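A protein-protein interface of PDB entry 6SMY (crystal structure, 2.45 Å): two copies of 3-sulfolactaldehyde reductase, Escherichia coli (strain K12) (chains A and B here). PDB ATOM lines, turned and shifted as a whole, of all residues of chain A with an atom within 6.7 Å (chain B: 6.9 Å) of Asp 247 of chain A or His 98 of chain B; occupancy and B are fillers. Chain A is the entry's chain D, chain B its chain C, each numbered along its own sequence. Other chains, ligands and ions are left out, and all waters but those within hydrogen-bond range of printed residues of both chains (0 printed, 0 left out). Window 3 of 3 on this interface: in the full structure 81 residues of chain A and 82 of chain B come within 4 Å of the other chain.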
ATOM      1  N   LEU A 242     -14.113 -14.331 -19.027  1.00  0.00           N
ATOM      2  CA  LEU A 242     -15.490 -14.830 -19.249  1.00  0.00           C
ATOM      3  C   LEU A 242     -15.441 -16.148 -20.036  1.00  0.00           C
ATOM      4  O   LEU A 242     -16.139 -17.082 -19.663  1.00  0.00           O
ATOM      5  CB  LEU A 242     -16.295 -13.767 -20.004  1.00  0.00           C
ATOM      6  CG  LEU A 242     -17.043 -12.744 -19.139  1.00  0.00           C
ATOM      7  CD1 LEU A 242     -18.001 -11.920 -19.974  1.00  0.00           C
ATOM      8  CD2 LEU A 242     -17.801 -13.416 -18.004  1.00  0.00           C
ATOM      9  N   GLY A 243     -14.608 -16.223 -21.067  1.00  0.00           N
ATOM     10  CA  GLY A 243     -14.353 -17.447 -21.852  1.00  0.00           C
ATOM     11  C   GLY A 243     -13.911 -18.602 -20.968  1.00  0.00           C
ATOM     12  O   GLY A 243     -14.486 -19.713 -21.077  1.00  0.00           O
ATOM     13  N   ILE A 244     -12.939 -18.354 -20.079  1.00  0.00           N
ATOM     14  CA  ILE A 244     -12.445 -19.414 -19.157  1.00  0.00           C
ATOM     15  C   ILE A 244     -13.617 -19.870 -18.286  1.00  0.00           C
ATOM     16  O   ILE A 244     -13.815 -21.095 -18.149  1.00  0.00           O
ATOM     17  CB  ILE A 244     -11.251 -18.933 -18.324  1.00  0.00           C
ATOM     18  CG1 ILE A 244     -10.037 -18.703 -19.223  1.00  0.00           C
ATOM     19  CG2 ILE A 244     -10.948 -19.930 -17.212  1.00  0.00           C
ATOM     20  CD1 ILE A 244      -9.006 -17.779 -18.611  1.00  0.00           C
ATOM     21  N   ALA A 245     -14.379 -18.926 -17.739  1.00  0.00           N
ATOM     22  CA  ALA A 245     -15.492 -19.215 -16.804  1.00  0.00           C
ATOM     23  C   ALA A 245     -16.514 -20.111 -17.507  1.00  0.00           C
ATOM     24  O   ALA A 245     -16.943 -21.134 -16.915  1.00  0.00           O
ATOM     25  CB  ALA A 245     -16.110 -17.939 -16.322  1.00  0.00           C
ATOM     26  N   LEU A 246     -16.825 -19.798 -18.758  1.00  0.00           N
ATOM     27  CA  LEU A 246     -17.871 -20.531 -19.511  1.00  0.00           C
ATOM     28  C   LEU A 246     -17.350 -21.912 -19.917  1.00  0.00           C
ATOM     29  O   LEU A 246     -18.164 -22.863 -19.844  1.00  0.00           O
ATOM     30  CB  LEU A 246     -18.325 -19.686 -20.693  1.00  0.00           C
ATOM     31  CG  LEU A 246     -19.240 -18.537 -20.281  1.00  0.00           C
ATOM     32  CD1 LEU A 246     -19.243 -17.429 -21.332  1.00  0.00           C
ATOM     33  CD2 LEU A 246     -20.646 -19.028 -19.987  1.00  0.00           C
ATOM     34  N   ASP A 247     -16.063 -22.027 -20.263  1.00  0.00           N
ATOM     35  CA  ASP A 247     -15.453 -23.341 -20.578  1.00  0.00           C
ATOM     36  C   ASP A 247     -15.552 -24.245 -19.338  1.00  0.00           C
ATOM     37  O   ASP A 247     -15.950 -25.408 -19.485  1.00  0.00           O
ATOM     38  CB  ASP A 247     -13.995 -23.243 -21.049  1.00  0.00           C
ATOM     39  CG  ASP A 247     -13.483 -24.566 -21.631  1.00  0.00           C
ATOM     40  OD1 ASP A 247     -14.223 -25.176 -22.440  1.00  0.00           O
ATOM     41  OD2 ASP A 247     -12.369 -25.041 -21.221  1.00  0.00           O
ATOM     42  N   VAL A 248     -15.197 -23.720 -18.167  1.00  0.00           N
ATOM     43  CA  VAL A 248     -15.178 -24.486 -16.887  1.00  0.00           C
ATOM     44  C   VAL A 248     -16.604 -24.909 -16.537  1.00  0.00           C
ATOM     45  O   VAL A 248     -16.827 -26.134 -16.342  1.00  0.00           O
ATOM     46  CB  VAL A 248     -14.518 -23.681 -15.756  1.00  0.00           C
ATOM     47  CG1 VAL A 248     -14.726 -24.318 -14.385  1.00  0.00           C
ATOM     48  CG2 VAL A 248     -13.040 -23.514 -16.035  1.00  0.00           C
ATOM     49  N   ALA A 249     -17.520 -23.945 -16.460  1.00  0.00           N
ATOM     50  CA  ALA A 249     -18.965 -24.193 -16.208  1.00  0.00           C
ATOM     51  C   ALA A 249     -19.476 -25.262 -17.187  1.00  0.00           C
ATOM     52  O   ALA A 249     -20.212 -26.162 -16.757  1.00  0.00           O
ATOM     53  CB  ALA A 249     -19.758 -22.903 -16.336  1.00  0.00           C
ATOM     54  N   ASN A 250     -19.100 -25.176 -18.463  1.00  0.00           N
ATOM     55  CA  ASN A 250     -19.596 -26.133 -19.489  1.00  0.00           C
ATOM     56  C   ASN A 250     -18.968 -27.510 -19.258  1.00  0.00           C
ATOM     57  O   ASN A 250     -19.692 -28.508 -19.467  1.00  0.00           O
ATOM     58  CB  ASN A 250     -19.471 -25.588 -20.909  1.00  0.00           C
ATOM     59  CG  ASN A 250     -20.682 -24.757 -21.283  1.00  0.00           C
ATOM     60  OD1 ASN A 250     -21.717 -25.299 -21.663  1.00  0.00           O
ATOM     61  ND2 ASN A 250     -20.604 -23.448 -21.118  1.00  0.00           N
ATOM     62  N   GLN A 251     -17.727 -27.599 -18.784  1.00  0.00           N
ATOM     63  CA  GLN A 251     -17.120 -28.925 -18.467  1.00  0.00           C
ATOM     64  C   GLN A 251     -17.800 -29.509 -17.209  1.00  0.00           C
ATOM     65  O   GLN A 251     -17.973 -30.724 -17.194  1.00  0.00           O
ATOM     66  CB  GLN A 251     -15.586 -28.840 -18.385  1.00  0.00           C
ATOM     67  CG  GLN A 251     -14.872 -30.188 -18.287  1.00  0.00           C
ATOM     68  CD  GLN A 251     -14.930 -30.802 -16.907  1.00  0.00           C
ATOM     69  OE1 GLN A 251     -14.975 -30.096 -15.899  1.00  0.00           O
ATOM     70  NE2 GLN A 251     -14.939 -32.133 -16.845  1.00  0.00           N
ATOM     71  N   LEU A 252     -18.229 -28.674 -16.246  1.00  0.00           N
ATOM     72  CA  LEU A 252     -18.858 -29.088 -14.964  1.00  0.00           C
ATOM     73  C   LEU A 252     -20.388 -29.142 -15.071  1.00  0.00           C
ATOM     74  O   LEU A 252     -21.026 -29.408 -14.049  1.00  0.00           O
ATOM     75  CB  LEU A 252     -18.439 -28.090 -13.877  1.00  0.00           C
ATOM     76  CG  LEU A 252     -16.947 -28.093 -13.564  1.00  0.00           C
ATOM     77  CD1 LEU A 252     -16.588 -27.077 -12.486  1.00  0.00           C
ATOM     78  CD2 LEU A 252     -16.538 -29.489 -13.113  1.00  0.00           C
ATOM     79  N   MET A 256     -24.932 -21.356 -17.159  1.00  0.00           N
ATOM     80  CA  MET A 256     -24.706 -19.932 -16.818  1.00  0.00           C
ATOM     81  C   MET A 256     -25.246 -19.048 -17.936  1.00  0.00           C
ATOM     82  O   MET A 256     -24.509 -18.403 -18.671  1.00  0.00           O
ATOM     83  CB  MET A 256     -23.217 -19.694 -16.553  1.00  0.00           C
ATOM     84  CG  MET A 256     -22.701 -20.576 -15.406  1.00  0.00           C
ATOM     85  SD  MET A 256     -21.362 -19.869 -14.465  1.00  0.00           S
ATOM     86  CE  MET A 256     -20.258 -19.376 -15.792  1.00  0.00           C
ATOM     87  N   ARG A 263     -20.882 -12.548 -22.203  1.00  0.00           N
ATOM     88  CA  ARG A 263     -19.670 -12.657 -23.033  1.00  0.00           C
ATOM     89  C   ARG A 263     -19.973 -12.099 -24.422  1.00  0.00           C
ATOM     90  O   ARG A 263     -19.080 -11.468 -24.994  1.00  0.00           O
ATOM     91  CB  ARG A 263     -19.131 -14.070 -23.148  1.00  0.00           C
ATOM     92  CG  ARG A 263     -17.909 -14.084 -24.050  1.00  0.00           C
ATOM     93  CD  ARG A 263     -17.130 -15.350 -24.079  1.00  0.00           C
ATOM     94  NE  ARG A 263     -17.841 -16.530 -24.530  1.00  0.00           N
ATOM     95  CZ  ARG A 263     -17.218 -17.621 -24.984  1.00  0.00           C
ATOM     96  NH1 ARG A 263     -15.895 -17.650 -25.091  1.00  0.00           N
ATOM     97  NH2 ARG A 263     -17.921 -18.666 -25.364  1.00  0.00           N
ATOM     98  N   ASN B  67      -2.557 -15.329 -20.773  1.00  0.00           N
ATOM     99  CA  ASN B  67      -3.211 -16.660 -20.920  1.00  0.00           C
ATOM    100  C   ASN B  67      -2.235 -17.796 -20.597  1.00  0.00           C
ATOM    101  O   ASN B  67      -0.997 -17.572 -20.592  1.00  0.00           O
ATOM    102  CB  ASN B  67      -3.801 -16.839 -22.322  1.00  0.00           C
ATOM    103  CG  ASN B  67      -2.763 -16.807 -23.425  1.00  0.00           C
ATOM    104  OD1 ASN B  67      -1.917 -17.697 -23.507  1.00  0.00           O
ATOM    105  ND2 ASN B  67      -2.824 -15.794 -24.281  1.00  0.00           N
ATOM    106  N   GLY B  68      -2.799 -18.986 -20.388  1.00  0.00           N
ATOM    107  CA  GLY B  68      -2.102 -20.202 -19.927  1.00  0.00           C
ATOM    108  C   GLY B  68      -1.184 -20.803 -20.972  1.00  0.00           C
ATOM    109  O   GLY B  68      -0.336 -21.609 -20.578  1.00  0.00           O
ATOM    110  N   THR B  96      -4.260 -14.759 -14.663  1.00  0.00           N
ATOM    111  CA  THR B  96      -5.626 -15.310 -14.795  1.00  0.00           C
ATOM    112  C   THR B  96      -5.630 -16.240 -16.007  1.00  0.00           C
ATOM    113  O   THR B  96      -5.642 -15.768 -17.139  1.00  0.00           O
ATOM    114  CB  THR B  96      -6.667 -14.197 -14.877  1.00  0.00           C
ATOM    115  OG1 THR B  96      -6.447 -13.322 -13.763  1.00  0.00           O
ATOM    116  CG2 THR B  96      -8.068 -14.777 -14.873  1.00  0.00           C
ATOM    117  N   ILE B  97      -5.583 -17.545 -15.755  1.00  0.00           N
ATOM    118  CA  ILE B  97      -5.622 -18.584 -16.819  1.00  0.00           C
ATOM    119  C   ILE B  97      -6.649 -19.633 -16.396  1.00  0.00           C
ATOM    120  O   ILE B  97      -7.246 -19.497 -15.295  1.00  0.00           O
ATOM    121  CB  ILE B  97      -4.223 -19.174 -17.043  1.00  0.00           C
ATOM    122  CG1 ILE B  97      -3.737 -20.011 -15.856  1.00  0.00           C
ATOM    123  CG2 ILE B  97      -3.246 -18.064 -17.375  1.00  0.00           C
ATOM    124  CD1 ILE B  97      -2.417 -20.732 -16.119  1.00  0.00           C
ATOM    125  N   HIS B  98      -6.849 -20.624 -17.257  1.00  0.00           N
ATOM    126  CA  HIS B  98      -7.811 -21.728 -17.061  1.00  0.00           C
ATOM    127  C   HIS B  98      -7.325 -22.533 -15.864  1.00  0.00           C
ATOM    128  O   HIS B  98      -6.165 -22.929 -15.824  1.00  0.00           O
ATOM    129  CB  HIS B  98      -7.931 -22.512 -18.375  1.00  0.00           C
ATOM    130  CG  HIS B  98      -9.104 -23.437 -18.441  1.00  0.00           C
ATOM    131  ND1 HIS B  98      -9.257 -24.460 -17.528  1.00  0.00           N
ATOM    132  CD2 HIS B  98     -10.145 -23.531 -19.312  1.00  0.00           C
ATOM    133  CE1 HIS B  98     -10.336 -25.171 -17.823  1.00  0.00           C
ATOM    134  NE2 HIS B  98     -10.910 -24.605 -18.920  1.00  0.00           N
ATOM    135  N   PRO B  99      -8.170 -22.800 -14.840  1.00  0.00           N
ATOM    136  CA  PRO B  99      -7.762 -23.602 -13.691  1.00  0.00           C
ATOM    137  C   PRO B  99      -7.105 -24.933 -14.067  1.00  0.00           C
ATOM    138  O   PRO B  99      -6.118 -25.283 -13.456  1.00  0.00           O
ATOM    139  CB  PRO B  99      -9.079 -23.875 -12.954  1.00  0.00           C
ATOM    140  CG  PRO B  99      -9.930 -22.686 -13.302  1.00  0.00           C
ATOM    141  CD  PRO B  99      -9.570 -22.370 -14.738  1.00  0.00           C
ATOM    142  N   LEU B 100      -7.679 -25.652 -15.031  1.00  0.00           N
ATOM    143  CA  LEU B 100      -7.125 -26.944 -15.508  1.00  0.00           C
ATOM    144  C   LEU B 100      -5.747 -26.703 -16.137  1.00  0.00           C
ATOM    145  O   LEU B 100      -4.907 -27.592 -15.996  1.00  0.00           O
ATOM    146  CB  LEU B 100      -8.088 -27.618 -16.492  1.00  0.00           C
ATOM    147  CG  LEU B 100      -9.097 -28.578 -15.855  1.00  0.00           C
ATOM    148  CD1 LEU B 100     -10.004 -27.856 -14.871  1.00  0.00           C
ATOM    149  CD2 LEU B 100      -9.913 -29.282 -16.932  1.00  0.00           C
ATOM    150  N   GLN B 101      -5.506 -25.551 -16.774  1.00  0.00           N
ATOM    151  CA  GLN B 101      -4.158 -25.209 -17.313  1.00  0.00           C
ATOM    152  C   GLN B 101      -3.166 -25.043 -16.142  1.00  0.00           C
ATOM    153  O   GLN B 101      -2.023 -25.524 -16.255  1.00  0.00           O
ATOM    154  CB  GLN B 101      -4.209 -23.968 -18.206  1.00  0.00           C
ATOM    155  CG  GLN B 101      -4.542 -24.269 -19.663  1.00  0.00           C
ATOM    156  CD  GLN B 101      -4.586 -23.020 -20.511  1.00  0.00           C
ATOM    157  OE1 GLN B 101      -4.992 -21.955 -20.065  1.00  0.00           O
ATOM    158  NE2 GLN B 101      -4.127 -23.111 -21.743  1.00  0.00           N
ATOM    159  N   THR B 102      -3.601 -24.412 -15.051  1.00  0.00           N
ATOM    160  CA  THR B 102      -2.815 -24.238 -13.801  1.00  0.00           C
ATOM    161  C   THR B 102      -2.486 -25.616 -13.191  1.00  0.00           C
ATOM    162  O   THR B 102      -1.306 -25.860 -12.919  1.00  0.00           O
ATOM    163  CB  THR B 102      -3.557 -23.328 -12.812  1.00  0.00           C
ATOM    164  OG1 THR B 102      -3.596 -22.027 -13.386  1.00  0.00           O
ATOM    165  CG2 THR B 102      -2.906 -23.257 -11.452  1.00  0.00           C
ATOM    166  N   ASP B 103      -3.488 -26.476 -12.977  1.00  0.00           N
ATOM    167  CA  ASP B 103      -3.324 -27.860 -12.445  1.00  0.00           C
ATOM    168  C   ASP B 103      -2.262 -28.628 -13.255  1.00  0.00           C
ATOM    169  O   ASP B 103      -1.386 -29.274 -12.620  1.00  0.00           O
ATOM    170  CB  ASP B 103      -4.646 -28.628 -12.464  1.00  0.00           C
ATOM    171  CG  ASP B 103      -5.689 -28.143 -11.462  1.00  0.00           C
ATOM    172  OD1 ASP B 103      -5.341 -27.352 -10.539  1.00  0.00           O
ATOM    173  OD2 ASP B 103      -6.865 -28.549 -11.616  1.00  0.00           O
ATOM    174  N   LEU B 105       0.130 -27.383 -15.250  1.00  0.00           N
ATOM    175  CA  LEU B 105       1.445 -26.703 -15.133  1.00  0.00           C
ATOM    176  C   LEU B 105       2.084 -27.049 -13.778  1.00  0.00           C
ATOM    177  O   LEU B 105       3.300 -27.296 -13.760  1.00  0.00           O
ATOM    178  CB  LEU B 105       1.261 -25.193 -15.312  1.00  0.00           C
ATOM    179  CG  LEU B 105       1.011 -24.739 -16.747  1.00  0.00           C
ATOM    180  CD1 LEU B 105       0.574 -23.288 -16.772  1.00  0.00           C
ATOM    181  CD2 LEU B 105       2.237 -24.936 -17.624  1.00  0.00           C
ATOM    182  N   ILE B 168      -6.465 -19.805  -8.380  1.00  0.00           N
ATOM    183  CA  ILE B 168      -7.051 -19.536  -9.719  1.00  0.00           C
ATOM    184  C   ILE B 168      -8.563 -19.824  -9.694  1.00  0.00           C
ATOM    185  O   ILE B 168      -9.318 -19.077 -10.331  1.00  0.00           O
ATOM    186  CB  ILE B 168      -6.292 -20.299 -10.817  1.00  0.00           C
ATOM    187  CG1 ILE B 168      -6.747 -19.853 -12.207  1.00  0.00           C
ATOM    188  CG2 ILE B 168      -6.387 -21.802 -10.622  1.00  0.00           C
ATOM    189  CD1 ILE B 168      -6.663 -18.338 -12.407  1.00  0.00           C
ATOM    190  N   ARG B 169      -9.008 -20.814  -8.936  1.00  0.00           N
ATOM    191  CA  ARG B 169     -10.448 -21.185  -8.852  1.00  0.00           C
ATOM    192  C   ARG B 169     -11.228 -20.005  -8.242  1.00  0.00           C
ATOM    193  O   ARG B 169     -12.239 -19.558  -8.857  1.00  0.00           O
ATOM    194  CB  ARG B 169     -10.627 -22.511  -8.107  1.00  0.00           C
ATOM    195  CG  ARG B 169     -10.326 -23.725  -8.990  1.00  0.00           C
ATOM    196  CD  ARG B 169     -10.155 -25.050  -8.270  1.00  0.00           C
ATOM    197  NE  ARG B 169     -10.099 -26.154  -9.227  1.00  0.00           N
ATOM    198  CZ  ARG B 169      -9.027 -26.493  -9.948  1.00  0.00           C
ATOM    199  NH1 ARG B 169      -7.906 -25.804  -9.836  1.00  0.00           N
ATOM    200  NH2 ARG B 169      -9.070 -27.516 -10.795  1.00  0.00           N
ATOM    201  N   LEU B 172     -11.381 -17.094 -10.608  1.00  0.00           N
ATOM    202  CA  LEU B 172     -12.389 -17.306 -11.682  1.00  0.00           C
ATOM    203  C   LEU B 172     -13.798 -16.937 -11.176  1.00  0.00           C
ATOM    204  O   LEU B 172     -14.500 -16.211 -11.884  1.00  0.00           O
ATOM    205  CB  LEU B 172     -12.319 -18.754 -12.161  1.00  0.00           C
ATOM    206  CG  LEU B 172     -13.106 -19.038 -13.440  1.00  0.00           C
ATOM    207  CD1 LEU B 172     -12.611 -18.191 -14.613  1.00  0.00           C
ATOM    208  CD2 LEU B 172     -13.001 -20.509 -13.823  1.00  0.00           C
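NE2 of His 98 of chain B lies within hydrogen-bond range of OD2 of Asp 247 of chain A, 2.8 Å away.
The backbone NH of Leu 100 of chain B sits at hydrogen-bond distance from a ring nitrogen (ND1) of His 98 of chain B (3.2 Å).
Among the printed residues, merely in contact across the chains: Ile 244 of chain A with Ile 97 of chain B, Ile 244 of chain A with His 98 of chain B, Ile 244 of chain A with Pro 99 of chain B, Ile 244 of chain A with Leu 172 of chain B, Ala 245 of chain A with Leu 172 of chain B, Val 248 of chain A with His 98 of chain B, Val 248 of chain A with Pro 99 of chain B and Val 248 of chain A with Leu 172 of chain B.
Asp 247 of chain A touches one residue of chain B. Thr 96 of chain B touches none of the printed residues of chain A. Of the printed residues of chain A, Ile 97 of chain B touches Ile 244 (3.7 Å). Of chain A, only Ile 244, Asp 247 and Val 248 come within 4 Å of His 98 of chain B. Asp 103 of chain B touches none of the printed residues of chain A. Printed residues of chain A within 4 Å of Leu 172 of chain B: Ile 244, Ala 245 and Val 248. The nearest printed residue of chain A that does not touch Pro 99 of chain B is Ala 245 of chain A (6.6 Å).
Of the 13 printed residues of chain A, 4 touch a printed residue of chain B. Hydrophobic or aromatic side chains of chain A within 4 Å of the printed part of chain B: Ile 244, Ala 245 and Val 248. Printed residues of chain B that touch a printed residue of chain A: Ile 97, His 98, Pro 99 and Leu 172. Among the printed residues, 9 pairs touch across the chains. Among the printed residues, no Asp or Glu carboxylate lies within 4 Å of a Lys or Arg side-chain nitrogen of the other chain.
No position is printed for both chains.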
